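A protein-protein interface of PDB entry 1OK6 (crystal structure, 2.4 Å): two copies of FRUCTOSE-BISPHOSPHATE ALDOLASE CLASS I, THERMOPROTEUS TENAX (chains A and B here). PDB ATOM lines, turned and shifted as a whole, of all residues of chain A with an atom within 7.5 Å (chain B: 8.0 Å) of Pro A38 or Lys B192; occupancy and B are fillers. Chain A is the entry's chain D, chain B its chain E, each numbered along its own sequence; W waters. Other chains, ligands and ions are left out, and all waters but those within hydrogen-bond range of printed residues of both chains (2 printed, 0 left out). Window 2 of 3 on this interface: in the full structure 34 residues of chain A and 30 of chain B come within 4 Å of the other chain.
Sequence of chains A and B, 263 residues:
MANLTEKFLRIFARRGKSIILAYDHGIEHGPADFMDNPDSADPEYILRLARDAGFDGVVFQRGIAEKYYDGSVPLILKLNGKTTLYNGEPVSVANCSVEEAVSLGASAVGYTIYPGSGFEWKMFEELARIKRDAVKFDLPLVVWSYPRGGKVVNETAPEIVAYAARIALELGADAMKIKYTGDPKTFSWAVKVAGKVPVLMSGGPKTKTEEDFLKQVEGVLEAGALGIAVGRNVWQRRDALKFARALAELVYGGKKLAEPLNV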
ATOM      1  N   TYR A  23     -16.401   0.790  15.896  1.00  0.00           N
ATOM      2  CA  TYR A  23     -17.701   0.307  16.298  1.00  0.00           C
ATOM      3  C   TYR A  23     -17.979   0.543  17.764  1.00  0.00           C
ATOM      4  O   TYR A  23     -18.637  -0.295  18.418  1.00  0.00           O
ATOM      5  CB  TYR A  23     -17.825  -1.186  15.983  1.00  0.00           C
ATOM      6  CG  TYR A  23     -19.231  -1.724  16.012  1.00  0.00           C
ATOM      7  CD1 TYR A  23     -20.244  -1.190  15.201  1.00  0.00           C
ATOM      8  CD2 TYR A  23     -19.549  -2.796  16.844  1.00  0.00           C
ATOM      9  CE1 TYR A  23     -21.564  -1.710  15.253  1.00  0.00           C
ATOM     10  CE2 TYR A  23     -20.837  -3.333  16.892  1.00  0.00           C
ATOM     11  CZ  TYR A  23     -21.846  -2.795  16.105  1.00  0.00           C
ATOM     12  OH  TYR A  23     -23.116  -3.379  16.182  1.00  0.00           O
ATOM     13  N   ASP A  33     -28.476   5.246  14.685  1.00  0.00           N
ATOM     14  CA  ASP A  33     -27.820   5.153  13.373  1.00  0.00           C
ATOM     15  C   ASP A  33     -27.783   3.723  12.781  1.00  0.00           C
ATOM     16  O   ASP A  33     -27.578   3.543  11.552  1.00  0.00           O
ATOM     17  CB  ASP A  33     -26.405   5.774  13.434  1.00  0.00           C
ATOM     18  CG  ASP A  33     -26.436   7.302  13.487  1.00  0.00           C
ATOM     19  OD1 ASP A  33     -27.420   7.906  13.001  1.00  0.00           O
ATOM     20  OD2 ASP A  33     -25.521   7.983  13.992  1.00  0.00           O
ATOM     21  N   PHE A  34     -27.996   2.724  13.647  1.00  0.00           N
ATOM     22  CA  PHE A  34     -28.067   1.331  13.219  1.00  0.00           C
ATOM     23  C   PHE A  34     -29.325   1.070  12.390  1.00  0.00           C
ATOM     24  O   PHE A  34     -29.414   0.044  11.716  1.00  0.00           O
ATOM     25  CB  PHE A  34     -28.036   0.354  14.407  1.00  0.00           C
ATOM     26  CG  PHE A  34     -26.759   0.381  15.218  1.00  0.00           C
ATOM     27  CD1 PHE A  34     -25.529   0.668  14.630  1.00  0.00           C
ATOM     28  CD2 PHE A  34     -26.797   0.093  16.579  1.00  0.00           C
ATOM     29  CE1 PHE A  34     -24.364   0.687  15.385  1.00  0.00           C
ATOM     30  CE2 PHE A  34     -25.646   0.110  17.347  1.00  0.00           C
ATOM     31  CZ  PHE A  34     -24.420   0.406  16.750  1.00  0.00           C
ATOM     32  N   MET A  35     -30.286   1.990  12.427  1.00  0.00           N
ATOM     33  CA  MET A  35     -31.584   1.761  11.769  1.00  0.00           C
ATOM     34  C   MET A  35     -31.531   1.782  10.227  1.00  0.00           C
ATOM     35  O   MET A  35     -32.268   1.044   9.568  1.00  0.00           O
ATOM     36  CB  MET A  35     -32.660   2.717  12.308  1.00  0.00           C
ATOM     37  CG  MET A  35     -33.132   2.369  13.721  1.00  0.00           C
ATOM     38  SD  MET A  35     -34.709   3.084  14.225  1.00  0.00           S
ATOM     39  CE  MET A  35     -35.871   2.219  13.146  1.00  0.00           C
ATOM     40  N   ASP A  36     -30.650   2.615   9.676  1.00  0.00           N
ATOM     41  CA  ASP A  36     -30.452   2.714   8.223  1.00  0.00           C
ATOM     42  C   ASP A  36     -30.058   1.384   7.562  1.00  0.00           C
ATOM     43  O   ASP A  36     -30.500   1.085   6.448  1.00  0.00           O
ATOM     44  CB  ASP A  36     -29.398   3.781   7.888  1.00  0.00           C
ATOM     45  CG  ASP A  36     -29.913   5.197   8.097  1.00  0.00           C
ATOM     46  OD1 ASP A  36     -30.669   5.435   9.068  1.00  0.00           O
ATOM     47  OD2 ASP A  36     -29.611   6.142   7.346  1.00  0.00           O
ATOM     48  N   ASN A  37     -29.217   0.618   8.258  1.00  0.00           N
ATOM     49  CA  ASN A  37     -28.775  -0.713   7.841  1.00  0.00           C
ATOM     50  C   ASN A  37     -28.817  -1.666   9.055  1.00  0.00           C
ATOM     51  O   ASN A  37     -27.798  -1.880   9.716  1.00  0.00           O
ATOM     52  CB  ASN A  37     -27.369  -0.625   7.207  1.00  0.00           C
ATOM     53  CG  ASN A  37     -26.829  -1.977   6.764  1.00  0.00           C
ATOM     54  OD1 ASN A  37     -27.536  -2.764   6.135  1.00  0.00           O
ATOM     55  ND2 ASN A  37     -25.567  -2.250   7.095  1.00  0.00           N
ATOM     56  N   PRO A  38     -30.000  -2.219   9.348  1.00  0.00           N
ATOM     57  CA  PRO A  38     -30.276  -2.909  10.625  1.00  0.00           C
ATOM     58  C   PRO A  38     -29.252  -3.948  11.090  1.00  0.00           C
ATOM     59  O   PRO A  38     -29.097  -4.098  12.299  1.00  0.00           O
ATOM     60  CB  PRO A  38     -31.620  -3.579  10.372  1.00  0.00           C
ATOM     61  CG  PRO A  38     -32.273  -2.712   9.381  1.00  0.00           C
ATOM     62  CD  PRO A  38     -31.178  -2.221   8.468  1.00  0.00           C
ATOM     63  N   ASP A  39     -28.588  -4.637  10.165  1.00  0.00           N
ATOM     64  CA  ASP A  39     -27.556  -5.625  10.485  1.00  0.00           C
ATOM     65  C   ASP A  39     -26.367  -5.030  11.271  1.00  0.00           C
ATOM     66  O   ASP A  39     -25.651  -5.752  11.975  1.00  0.00           O
ATOM     67  CB  ASP A  39     -27.031  -6.278   9.193  1.00  0.00           C
ATOM     68  CG  ASP A  39     -28.007  -7.283   8.577  1.00  0.00           C
ATOM     69  OD1 ASP A  39     -28.882  -7.847   9.281  1.00  0.00           O
ATOM     70  OD2 ASP A  39     -27.942  -7.589   7.374  1.00  0.00           O
ATOM     71  N   SER A  40     -26.166  -3.718  11.140  1.00  0.00           N
ATOM     72  CA  SER A  40     -25.062  -3.034  11.785  1.00  0.00           C
ATOM     73  C   SER A  40     -25.210  -3.023  13.301  1.00  0.00           C
ATOM     74  O   SER A  40     -24.220  -2.824  14.008  1.00  0.00           O
ATOM     75  CB  SER A  40     -24.891  -1.617  11.238  1.00  0.00           C
ATOM     76  OG  SER A  40     -26.062  -0.853  11.416  1.00  0.00           O
ATOM     77  N   ALA A  41     -26.432  -3.245  13.797  1.00  0.00           N
ATOM     78  CA  ALA A  41     -26.666  -3.423  15.235  1.00  0.00           C
ATOM     79  C   ALA A  41     -26.053  -4.721  15.762  1.00  0.00           C
ATOM     80  O   ALA A  41     -25.821  -4.865  16.967  1.00  0.00           O
ATOM     81  CB  ALA A  41     -28.143  -3.361  15.548  1.00  0.00           C
ATOM     82  N   ASP A  42     -25.773  -5.649  14.852  1.00  0.00           N
ATOM     83  CA  ASP A  42     -25.174  -6.939  15.178  1.00  0.00           C
ATOM     84  C   ASP A  42     -23.641  -6.911  15.055  1.00  0.00           C
ATOM     85  O   ASP A  42     -23.116  -6.789  13.952  1.00  0.00           O
ATOM     86  CB  ASP A  42     -25.765  -7.994  14.235  1.00  0.00           C
ATOM     87  CG  ASP A  42     -25.331  -9.416  14.561  1.00  0.00           C
ATOM     88  OD1 ASP A  42     -24.757  -9.688  15.652  1.00  0.00           O
ATOM     89  OD2 ASP A  42     -25.554 -10.350  13.751  1.00  0.00           O
ATOM     90  N   PRO A  43     -22.918  -7.042  16.167  1.00  0.00           N
ATOM     91  CA  PRO A  43     -21.447  -7.033  16.123  1.00  0.00           C
ATOM     92  C   PRO A  43     -20.855  -8.157  15.270  1.00  0.00           C
ATOM     93  O   PRO A  43     -19.772  -7.981  14.723  1.00  0.00           O
ATOM     94  CB  PRO A  43     -21.047  -7.179  17.593  1.00  0.00           C
ATOM     95  CG  PRO A  43     -22.245  -6.720  18.356  1.00  0.00           C
ATOM     96  CD  PRO A  43     -23.424  -7.208  17.543  1.00  0.00           C
ATOM     97  N   TYR A  45     -22.019  -9.215  12.442  1.00  0.00           N
ATOM     98  CA  TYR A  45     -22.041  -8.661  11.103  1.00  0.00           C
ATOM     99  C   TYR A  45     -20.820  -7.776  10.846  1.00  0.00           C
ATOM    100  O   TYR A  45     -20.247  -7.814   9.753  1.00  0.00           O
ATOM    101  CB  TYR A  45     -23.358  -7.894  10.893  1.00  0.00           C
ATOM    102  CG  TYR A  45     -23.376  -6.940   9.725  1.00  0.00           C
ATOM    103  CD1 TYR A  45     -23.581  -7.408   8.405  1.00  0.00           C
ATOM    104  CD2 TYR A  45     -23.215  -5.569   9.921  1.00  0.00           C
ATOM    105  CE1 TYR A  45     -23.604  -6.522   7.335  1.00  0.00           C
ATOM    106  CE2 TYR A  45     -23.237  -4.679   8.841  1.00  0.00           C
ATOM    107  CZ  TYR A  45     -23.425  -5.160   7.581  1.00  0.00           C
ATOM    108  OH  TYR A  45     -23.439  -4.254   6.567  1.00  0.00           O
ATOM    109  N   TYR A  68     -18.763 -10.848  21.859  1.00  0.00           N
ATOM    110  CA  TYR A  68     -18.702 -11.156  20.420  1.00  0.00           C
ATOM    111  C   TYR A  68     -17.328 -11.429  19.792  1.00  0.00           C
ATOM    112  O   TYR A  68     -17.250 -12.072  18.754  1.00  0.00           O
ATOM    113  CB  TYR A  68     -19.410 -10.064  19.595  1.00  0.00           C
ATOM    114  CG  TYR A  68     -20.903  -9.972  19.844  1.00  0.00           C
ATOM    115  CD1 TYR A  68     -21.813 -10.600  18.995  1.00  0.00           C
ATOM    116  CD2 TYR A  68     -21.406  -9.241  20.927  1.00  0.00           C
ATOM    117  CE1 TYR A  68     -23.196 -10.514  19.217  1.00  0.00           C
ATOM    118  CE2 TYR A  68     -22.778  -9.160  21.164  1.00  0.00           C
ATOM    119  CZ  TYR A  68     -23.673  -9.794  20.304  1.00  0.00           C
ATOM    120  OH  TYR A  68     -25.031  -9.704  20.538  1.00  0.00           O
ATOM    121  N   TRP A 235     -20.588   0.973   7.714  1.00  0.00           N
ATOM    122  CA  TRP A 235     -21.697   0.130   8.179  1.00  0.00           C
ATOM    123  C   TRP A 235     -23.110   0.743   8.213  1.00  0.00           C
ATOM    124  O   TRP A 235     -24.094   0.023   8.382  1.00  0.00           O
ATOM    125  CB  TRP A 235     -21.365  -0.568   9.492  1.00  0.00           C
ATOM    126  CG  TRP A 235     -20.929   0.315  10.625  1.00  0.00           C
ATOM    127  CD1 TRP A 235     -19.680   0.376  11.184  1.00  0.00           C
ATOM    128  CD2 TRP A 235     -21.743   1.225  11.372  1.00  0.00           C
ATOM    129  NE1 TRP A 235     -19.665   1.271  12.222  1.00  0.00           N
ATOM    130  CE2 TRP A 235     -20.922   1.808  12.362  1.00  0.00           C
ATOM    131  CE3 TRP A 235     -23.094   1.600  11.316  1.00  0.00           C
ATOM    132  CZ2 TRP A 235     -21.406   2.757  13.282  1.00  0.00           C
ATOM    133  CZ3 TRP A 235     -23.572   2.536  12.212  1.00  0.00           C
ATOM    134  CH2 TRP A 235     -22.731   3.105  13.189  1.00  0.00           C
ATOM    135  N   GLN A 236     -23.219   2.056   8.038  1.00  0.00           N
ATOM    136  CA  GLN A 236     -24.531   2.694   7.922  1.00  0.00           C
ATOM    137  C   GLN A 236     -25.097   2.557   6.500  1.00  0.00           C
ATOM    138  O   GLN A 236     -26.290   2.796   6.279  1.00  0.00           O
ATOM    139  CB  GLN A 236     -24.466   4.169   8.327  1.00  0.00           C
ATOM    140  CG  GLN A 236     -25.792   4.747   8.798  1.00  0.00           C
ATOM    141  CD  GLN A 236     -25.664   6.155   9.392  1.00  0.00           C
ATOM    142  OE1 GLN A 236     -24.576   6.583   9.828  1.00  0.00           O
ATOM    143  NE2 GLN A 236     -26.784   6.876   9.422  1.00  0.00           N
ATOM    144  N   ALA B 162     -33.993   2.145  23.891  1.00  0.00           N
ATOM    145  CA  ALA B 162     -33.010   1.525  23.009  1.00  0.00           C
ATOM    146  C   ALA B 162     -31.566   1.901  23.392  1.00  0.00           C
ATOM    147  O   ALA B 162     -30.684   1.042  23.436  1.00  0.00           O
ATOM    148  CB  ALA B 162     -33.287   1.870  21.523  1.00  0.00           C
ATOM    149  N   ALA B 165     -30.529   0.075  26.518  1.00  0.00           N
ATOM    150  CA  ALA B 165     -30.242  -1.335  26.273  1.00  0.00           C
ATOM    151  C   ALA B 165     -28.852  -1.507  25.663  1.00  0.00           C
ATOM    152  O   ALA B 165     -28.090  -2.402  26.048  1.00  0.00           O
ATOM    153  CB  ALA B 165     -31.341  -1.970  25.348  1.00  0.00           C
ATOM    154  N   ARG B 166     -28.519  -0.637  24.711  1.00  0.00           N
ATOM    155  CA  ARG B 166     -27.250  -0.742  24.014  1.00  0.00           C
ATOM    156  C   ARG B 166     -26.097  -0.402  24.958  1.00  0.00           C
ATOM    157  O   ARG B 166     -25.079  -1.100  24.969  1.00  0.00           O
ATOM    158  CB  ARG B 166     -27.224   0.149  22.779  1.00  0.00           C
ATOM    159  CG  ARG B 166     -26.024  -0.088  21.845  1.00  0.00           C
ATOM    160  CD  ARG B 166     -25.679  -1.548  21.663  1.00  0.00           C
ATOM    161  NE  ARG B 166     -24.605  -1.705  20.705  1.00  0.00           N
ATOM    162  CZ  ARG B 166     -24.677  -2.446  19.600  1.00  0.00           C
ATOM    163  NH1 ARG B 166     -25.790  -3.132  19.326  1.00  0.00           N
ATOM    164  NH2 ARG B 166     -23.629  -2.496  18.774  1.00  0.00           N
ATOM    165  N   LEU B 169     -25.188  -3.313  27.156  1.00  0.00           N
ATOM    166  CA  LEU B 169     -24.404  -4.297  26.408  1.00  0.00           C
ATOM    167  C   LEU B 169     -22.926  -3.859  26.275  1.00  0.00           C
ATOM    168  O   LEU B 169     -21.979  -4.642  26.532  1.00  0.00           O
ATOM    169  CB  LEU B 169     -25.045  -4.564  25.027  1.00  0.00           C
ATOM    170  CG  LEU B 169     -24.200  -5.294  23.979  1.00  0.00           C
ATOM    171  CD1 LEU B 169     -23.944  -6.755  24.359  1.00  0.00           C
ATOM    172  CD2 LEU B 169     -24.849  -5.213  22.619  1.00  0.00           C
ATOM    173  N   LYS B 185     -43.640  -3.196  19.597  1.00  0.00           N
ATOM    174  CA  LYS B 185     -42.848  -2.927  18.410  1.00  0.00           C
ATOM    175  C   LYS B 185     -41.541  -2.194  18.755  1.00  0.00           C
ATOM    176  O   LYS B 185     -40.447  -2.673  18.433  1.00  0.00           O
ATOM    177  CB  LYS B 185     -43.661  -2.170  17.358  1.00  0.00           C
ATOM    178  CG  LYS B 185     -43.357  -2.585  15.917  1.00  0.00           C
ATOM    179  CD  LYS B 185     -44.198  -1.796  14.886  1.00  0.00           C
ATOM    180  CE  LYS B 185     -43.342  -1.347  13.678  1.00  0.00           C
ATOM    181  NZ  LYS B 185     -41.903  -1.141  14.046  1.00  0.00           N
ATOM    182  N   THR B 186     -41.641  -1.057  19.438  1.00  0.00           N
ATOM    183  CA  THR B 186     -40.439  -0.285  19.778  1.00  0.00           C
ATOM    184  C   THR B 186     -39.576  -0.995  20.817  1.00  0.00           C
ATOM    185  O   THR B 186     -38.347  -0.889  20.777  1.00  0.00           O
ATOM    186  CB  THR B 186     -40.793   1.125  20.269  1.00  0.00           C
ATOM    187  OG1 THR B 186     -41.731   1.033  21.364  1.00  0.00           O
ATOM    188  CG2 THR B 186     -41.516   1.922  19.164  1.00  0.00           C
ATOM    189  N   PHE B 187     -40.205  -1.720  21.742  1.00  0.00           N
ATOM    190  CA  PHE B 187     -39.451  -2.451  22.748  1.00  0.00           C
ATOM    191  C   PHE B 187     -38.614  -3.554  22.125  1.00  0.00           C
ATOM    192  O   PHE B 187     -37.526  -3.851  22.622  1.00  0.00           O
ATOM    193  CB  PHE B 187     -40.348  -3.022  23.839  1.00  0.00           C
ATOM    194  CG  PHE B 187     -39.608  -3.401  25.100  1.00  0.00           C
ATOM    195  CD1 PHE B 187     -39.091  -2.421  25.953  1.00  0.00           C
ATOM    196  CD2 PHE B 187     -39.438  -4.734  25.441  1.00  0.00           C
ATOM    197  CE1 PHE B 187     -38.417  -2.767  27.128  1.00  0.00           C
ATOM    198  CE2 PHE B 187     -38.780  -5.097  26.607  1.00  0.00           C
ATOM    199  CZ  PHE B 187     -38.256  -4.107  27.455  1.00  0.00           C
ATOM    200  N   SER B 188     -39.086  -4.140  21.027  1.00  0.00           N
ATOM    201  CA  SER B 188     -38.307  -5.188  20.390  1.00  0.00           C
ATOM    202  C   SER B 188     -37.070  -4.663  19.656  1.00  0.00           C
ATOM    203  O   SER B 188     -36.134  -5.428  19.437  1.00  0.00           O
ATOM    204  CB  SER B 188     -39.168  -6.028  19.468  1.00  0.00           C
ATOM    205  OG  SER B 188     -39.659  -5.204  18.454  1.00  0.00           O
ATOM    206  N   TRP B 189     -37.043  -3.376  19.296  1.00  0.00           N
ATOM    207  CA  TRP B 189     -35.791  -2.744  18.842  1.00  0.00           C
ATOM    208  C   TRP B 189     -34.771  -2.620  19.993  1.00  0.00           C
ATOM    209  O   TRP B 189     -33.565  -2.811  19.795  1.00  0.00           O
ATOM    210  CB  TRP B 189     -36.041  -1.373  18.168  1.00  0.00           C
ATOM    211  CG  TRP B 189     -34.778  -0.602  17.738  1.00  0.00           C
ATOM    212  CD1 TRP B 189     -34.324   0.595  18.251  1.00  0.00           C
ATOM    213  CD2 TRP B 189     -33.834  -0.977  16.727  1.00  0.00           C
ATOM    214  NE1 TRP B 189     -33.161   0.979  17.620  1.00  0.00           N
ATOM    215  CE2 TRP B 189     -32.840   0.039  16.674  1.00  0.00           C
ATOM    216  CE3 TRP B 189     -33.726  -2.062  15.847  1.00  0.00           C
ATOM    217  CZ2 TRP B 189     -31.758  -0.004  15.779  1.00  0.00           C
ATOM    218  CZ3 TRP B 189     -32.640  -2.100  14.954  1.00  0.00           C
ATOM    219  CH2 TRP B 189     -31.669  -1.076  14.939  1.00  0.00           C
ATOM    220  N   ALA B 190     -35.256  -2.304  21.194  1.00  0.00           N
ATOM    221  CA  ALA B 190     -34.386  -2.272  22.367  1.00  0.00           C
ATOM    222  C   ALA B 190     -33.808  -3.675  22.616  1.00  0.00           C
ATOM    223  O   ALA B 190     -32.601  -3.833  22.808  1.00  0.00           O
ATOM    224  CB  ALA B 190     -35.151  -1.768  23.581  1.00  0.00           C
ATOM    225  N   VAL B 191     -34.674  -4.692  22.563  1.00  0.00           N
ATOM    226  CA  VAL B 191     -34.258  -6.091  22.715  1.00  0.00           C
ATOM    227  C   VAL B 191     -33.235  -6.471  21.621  1.00  0.00           C
ATOM    228  O   VAL B 191     -32.235  -7.151  21.892  1.00  0.00           O
ATOM    229  CB  VAL B 191     -35.472  -7.043  22.713  1.00  0.00           C
ATOM    230  CG1 VAL B 191     -35.041  -8.501  22.616  1.00  0.00           C
ATOM    231  CG2 VAL B 191     -36.342  -6.815  23.961  1.00  0.00           C
ATOM    232  N   LYS B 192     -33.475  -6.004  20.402  1.00  0.00           N
ATOM    233  CA  LYS B 192     -32.579  -6.326  19.298  1.00  0.00           C
ATOM    234  C   LYS B 192     -31.181  -5.729  19.453  1.00  0.00           C
ATOM    235  O   LYS B 192     -30.199  -6.386  19.125  1.00  0.00           O
ATOM    236  CB  LYS B 192     -33.176  -5.926  17.933  1.00  0.00           C
ATOM    237  CG  LYS B 192     -32.175  -5.983  16.767  1.00  0.00           C
ATOM    238  CD  LYS B 192     -32.096  -7.369  16.098  1.00  0.00           C
ATOM    239  CE  LYS B 192     -32.253  -7.283  14.549  1.00  0.00           C
ATOM    240  NZ  LYS B 192     -31.007  -6.850  13.853  1.00  0.00           N
ATOM    241  N   VAL B 193     -31.091  -4.501  19.944  1.00  0.00           N
ATOM    242  CA  VAL B 193     -29.783  -3.864  20.084  1.00  0.00           C
ATOM    243  C   VAL B 193     -29.012  -4.384  21.306  1.00  0.00           C
ATOM    244  O   VAL B 193     -27.803  -4.231  21.399  1.00  0.00           O
ATOM    245  CB  VAL B 193     -29.865  -2.318  20.058  1.00  0.00           C
ATOM    246  CG1 VAL B 193     -30.472  -1.826  18.714  1.00  0.00           C
ATOM    247  CG2 VAL B 193     -30.625  -1.792  21.277  1.00  0.00           C
ATOM    248  N   ALA B 194     -29.723  -5.036  22.215  1.00  0.00           N
ATOM    249  CA  ALA B 194     -29.102  -5.728  23.346  1.00  0.00           C
ATOM    250  C   ALA B 194     -28.338  -6.978  22.930  1.00  0.00           C
ATOM    251  O   ALA B 194     -27.516  -7.480  23.687  1.00  0.00           O
ATOM    252  CB  ALA B 194     -30.141  -6.083  24.382  1.00  0.00           C
ATOM    253  N   GLY B 195     -28.628  -7.490  21.734  1.00  0.00           N
ATOM    254  CA  GLY B 195     -27.925  -8.636  21.187  1.00  0.00           C
ATOM    255  C   GLY B 195     -28.039  -9.878  22.044  1.00  0.00           C
ATOM    256  O   GLY B 195     -29.138 -10.277  22.420  1.00  0.00           O
ATOM    257  N   LYS B 196     -26.899 -10.482  22.359  1.00  0.00           N
ATOM    258  CA  LYS B 196     -26.823 -11.701  23.175  1.00  0.00           C
ATOM    259  C   LYS B 196     -27.216 -11.481  24.627  1.00  0.00           C
ATOM    260  O   LYS B 196     -27.378 -12.461  25.358  1.00  0.00           O
ATOM    261  CB  LYS B 196     -25.380 -12.204  23.221  1.00  0.00           C
ATOM    262  CG  LYS B 196     -24.997 -13.190  22.155  1.00  0.00           C
ATOM    263  CD  LYS B 196     -23.479 -13.263  22.070  1.00  0.00           C
ATOM    264  CE  LYS B 196     -23.059 -13.962  20.805  1.00  0.00           C
ATOM    265  NZ  LYS B 196     -21.656 -14.429  20.930  1.00  0.00           N
ATOM    266  N   VAL B 197     -27.321 -10.223  25.069  1.00  0.00           N
ATOM    267  CA  VAL B 197     -27.638  -9.955  26.479  1.00  0.00           C
ATOM    268  C   VAL B 197     -29.152  -9.916  26.755  1.00  0.00           C
ATOM    269  O   VAL B 197     -29.862  -9.083  26.180  1.00  0.00           O
ATOM    270  CB  VAL B 197     -26.939  -8.677  26.981  1.00  0.00           C
ATOM    271  CG1 VAL B 197     -27.264  -8.401  28.433  1.00  0.00           C
ATOM    272  CG2 VAL B 197     -25.452  -8.825  26.836  1.00  0.00           C
ATOM    273  N   VAL B 199     -32.874  -9.271  28.257  1.00  0.00           N
ATOM    274  CA  VAL B 199     -33.504  -8.060  28.739  1.00  0.00           C
ATOM    275  C   VAL B 199     -34.679  -8.403  29.636  1.00  0.00           C
ATOM    276  O   VAL B 199     -35.569  -9.170  29.230  1.00  0.00           O
ATOM    277  CB  VAL B 199     -34.030  -7.243  27.561  1.00  0.00           C
ATOM    278  CG1 VAL B 199     -34.954  -6.133  28.037  1.00  0.00           C
ATOM    279  CG2 VAL B 199     -32.884  -6.688  26.737  1.00  0.00           C
ATOM    280  N   ALA B 223     -42.052  -8.998  22.390  1.00  0.00           N
ATOM    281  CA  ALA B 223     -40.888  -8.279  21.908  1.00  0.00           C
ATOM    282  C   ALA B 223     -39.615  -9.121  22.009  1.00  0.00           C
ATOM    283  O   ALA B 223     -38.590  -8.750  21.443  1.00  0.00           O
ATOM    284  CB  ALA B 223     -40.743  -6.980  22.686  1.00  0.00           C
ATOM    285  N   GLY B 224     -39.672 -10.241  22.731  1.00  0.00           N
ATOM    286  CA  GLY B 224     -38.542 -11.149  22.859  1.00  0.00           C
ATOM    287  C   GLY B 224     -37.681 -10.954  24.100  1.00  0.00           C
ATOM    288  O   GLY B 224     -36.556 -11.464  24.163  1.00  0.00           O
ATOM    289  N   ALA B 225     -38.193 -10.210  25.077  1.00  0.00           N
ATOM    290  CA  ALA B 225     -37.528 -10.076  26.366  1.00  0.00           C
ATOM    291  C   ALA B 225     -37.514 -11.410  27.120  1.00  0.00           C
ATOM    292  O   ALA B 225     -38.371 -12.264  26.913  1.00  0.00           O
ATOM    293  CB  ALA B 225     -38.206  -8.990  27.195  1.00  0.00           C
HETATM  294  O   HOH W   1     -27.694  -6.968  17.962  1.00  0.00           O
HETATM  295  O   HOH W   2     -21.243  -0.295  19.025  1.00  0.00           O
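No position is printed for both chains. Of the 8 pairs that touch across the chains among the printed residues, none has its exchanged pair printed and touching as well.
Phe A34 touches Arg B166 (CE2 to CZ, 3.5 Å). Phe A34 touches Trp B189. CG of Met A35 touches CZ2 of Trp B189, at 3.4 Å. O of Pro A38 touches NZ of Lys B192, 3.7 Å away. Tyr A68 touches Gly B195 (OH to CA, 3.2 Å).
NH1 of Arg B166 lies within hydrogen-bond range of O of Ala A41, at 2.9 Å. OH of Tyr A23 sits at hydrogen-bond distance from NH2 of Arg B166. N of Lys B196 sits at hydrogen-bond distance from OH of Tyr A68.
OH of Tyr A23 is in hydrogen-bond range of O of Ala A41 (3.2 Å). NH1 of Arg B166 is in hydrogen-bond range of O of Val B193 (3.1 Å). The backbone carbonyl oxygen (O) of Phe A34 sits close to the side-chain hydroxyl (OG) of Ser A40 (3.5 Å). O of Ser A40 is in hydrogen-bond range of OH of Tyr A23, at 2.5 Å.
Of the 16 printed residues of chain A, 6 touch a printed residue of chain B. Hydrophobic or aromatic side chains of chain A within 4 Å of the printed part of chain B: Tyr A23, Phe A34, Met A35 and Tyr A68. Among the printed residues, 8 pairs touch across the chains. Among the printed residues, no Asp or Glu carboxylate lies within 4 Å of a Lys or Arg side-chain nitrogen of the other chain.
Of the printed residues of chain B, Tyr A23 touches Arg B166. Printed residues of chain B within 4 Å of Phe A34: Arg B166 and Trp B189. Printed residues of chain B within 4 Å of Pro A38: Lys B192. Of the printed residues of chain B, Ala A41 touches Arg B166. Of the printed residues of chain B, Tyr A68 touches Gly B195 (3.2 Å) and Lys B196 (2.7 Å). Lys B192 touches one residue of chain A. Printed residues of chain A within 4 Å of Gly B195: Tyr A68. The nearest residue of chain B that does not touch Pro A38 is Trp B189 (4.8 Å). The nearest printed residue of chain B that does not touch Tyr A23 is Leu B169 (6.9 Å).
Water W2 lies within hydrogen-bond range of the backbone carbonyl oxygen (O) of Tyr A23 (2.7 Å) and the guanidinium group (NH2) of Arg B166 (3.3 Å). Water W1 lies within hydrogen-bond range of O of Lys B192 and O of Ala A41.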
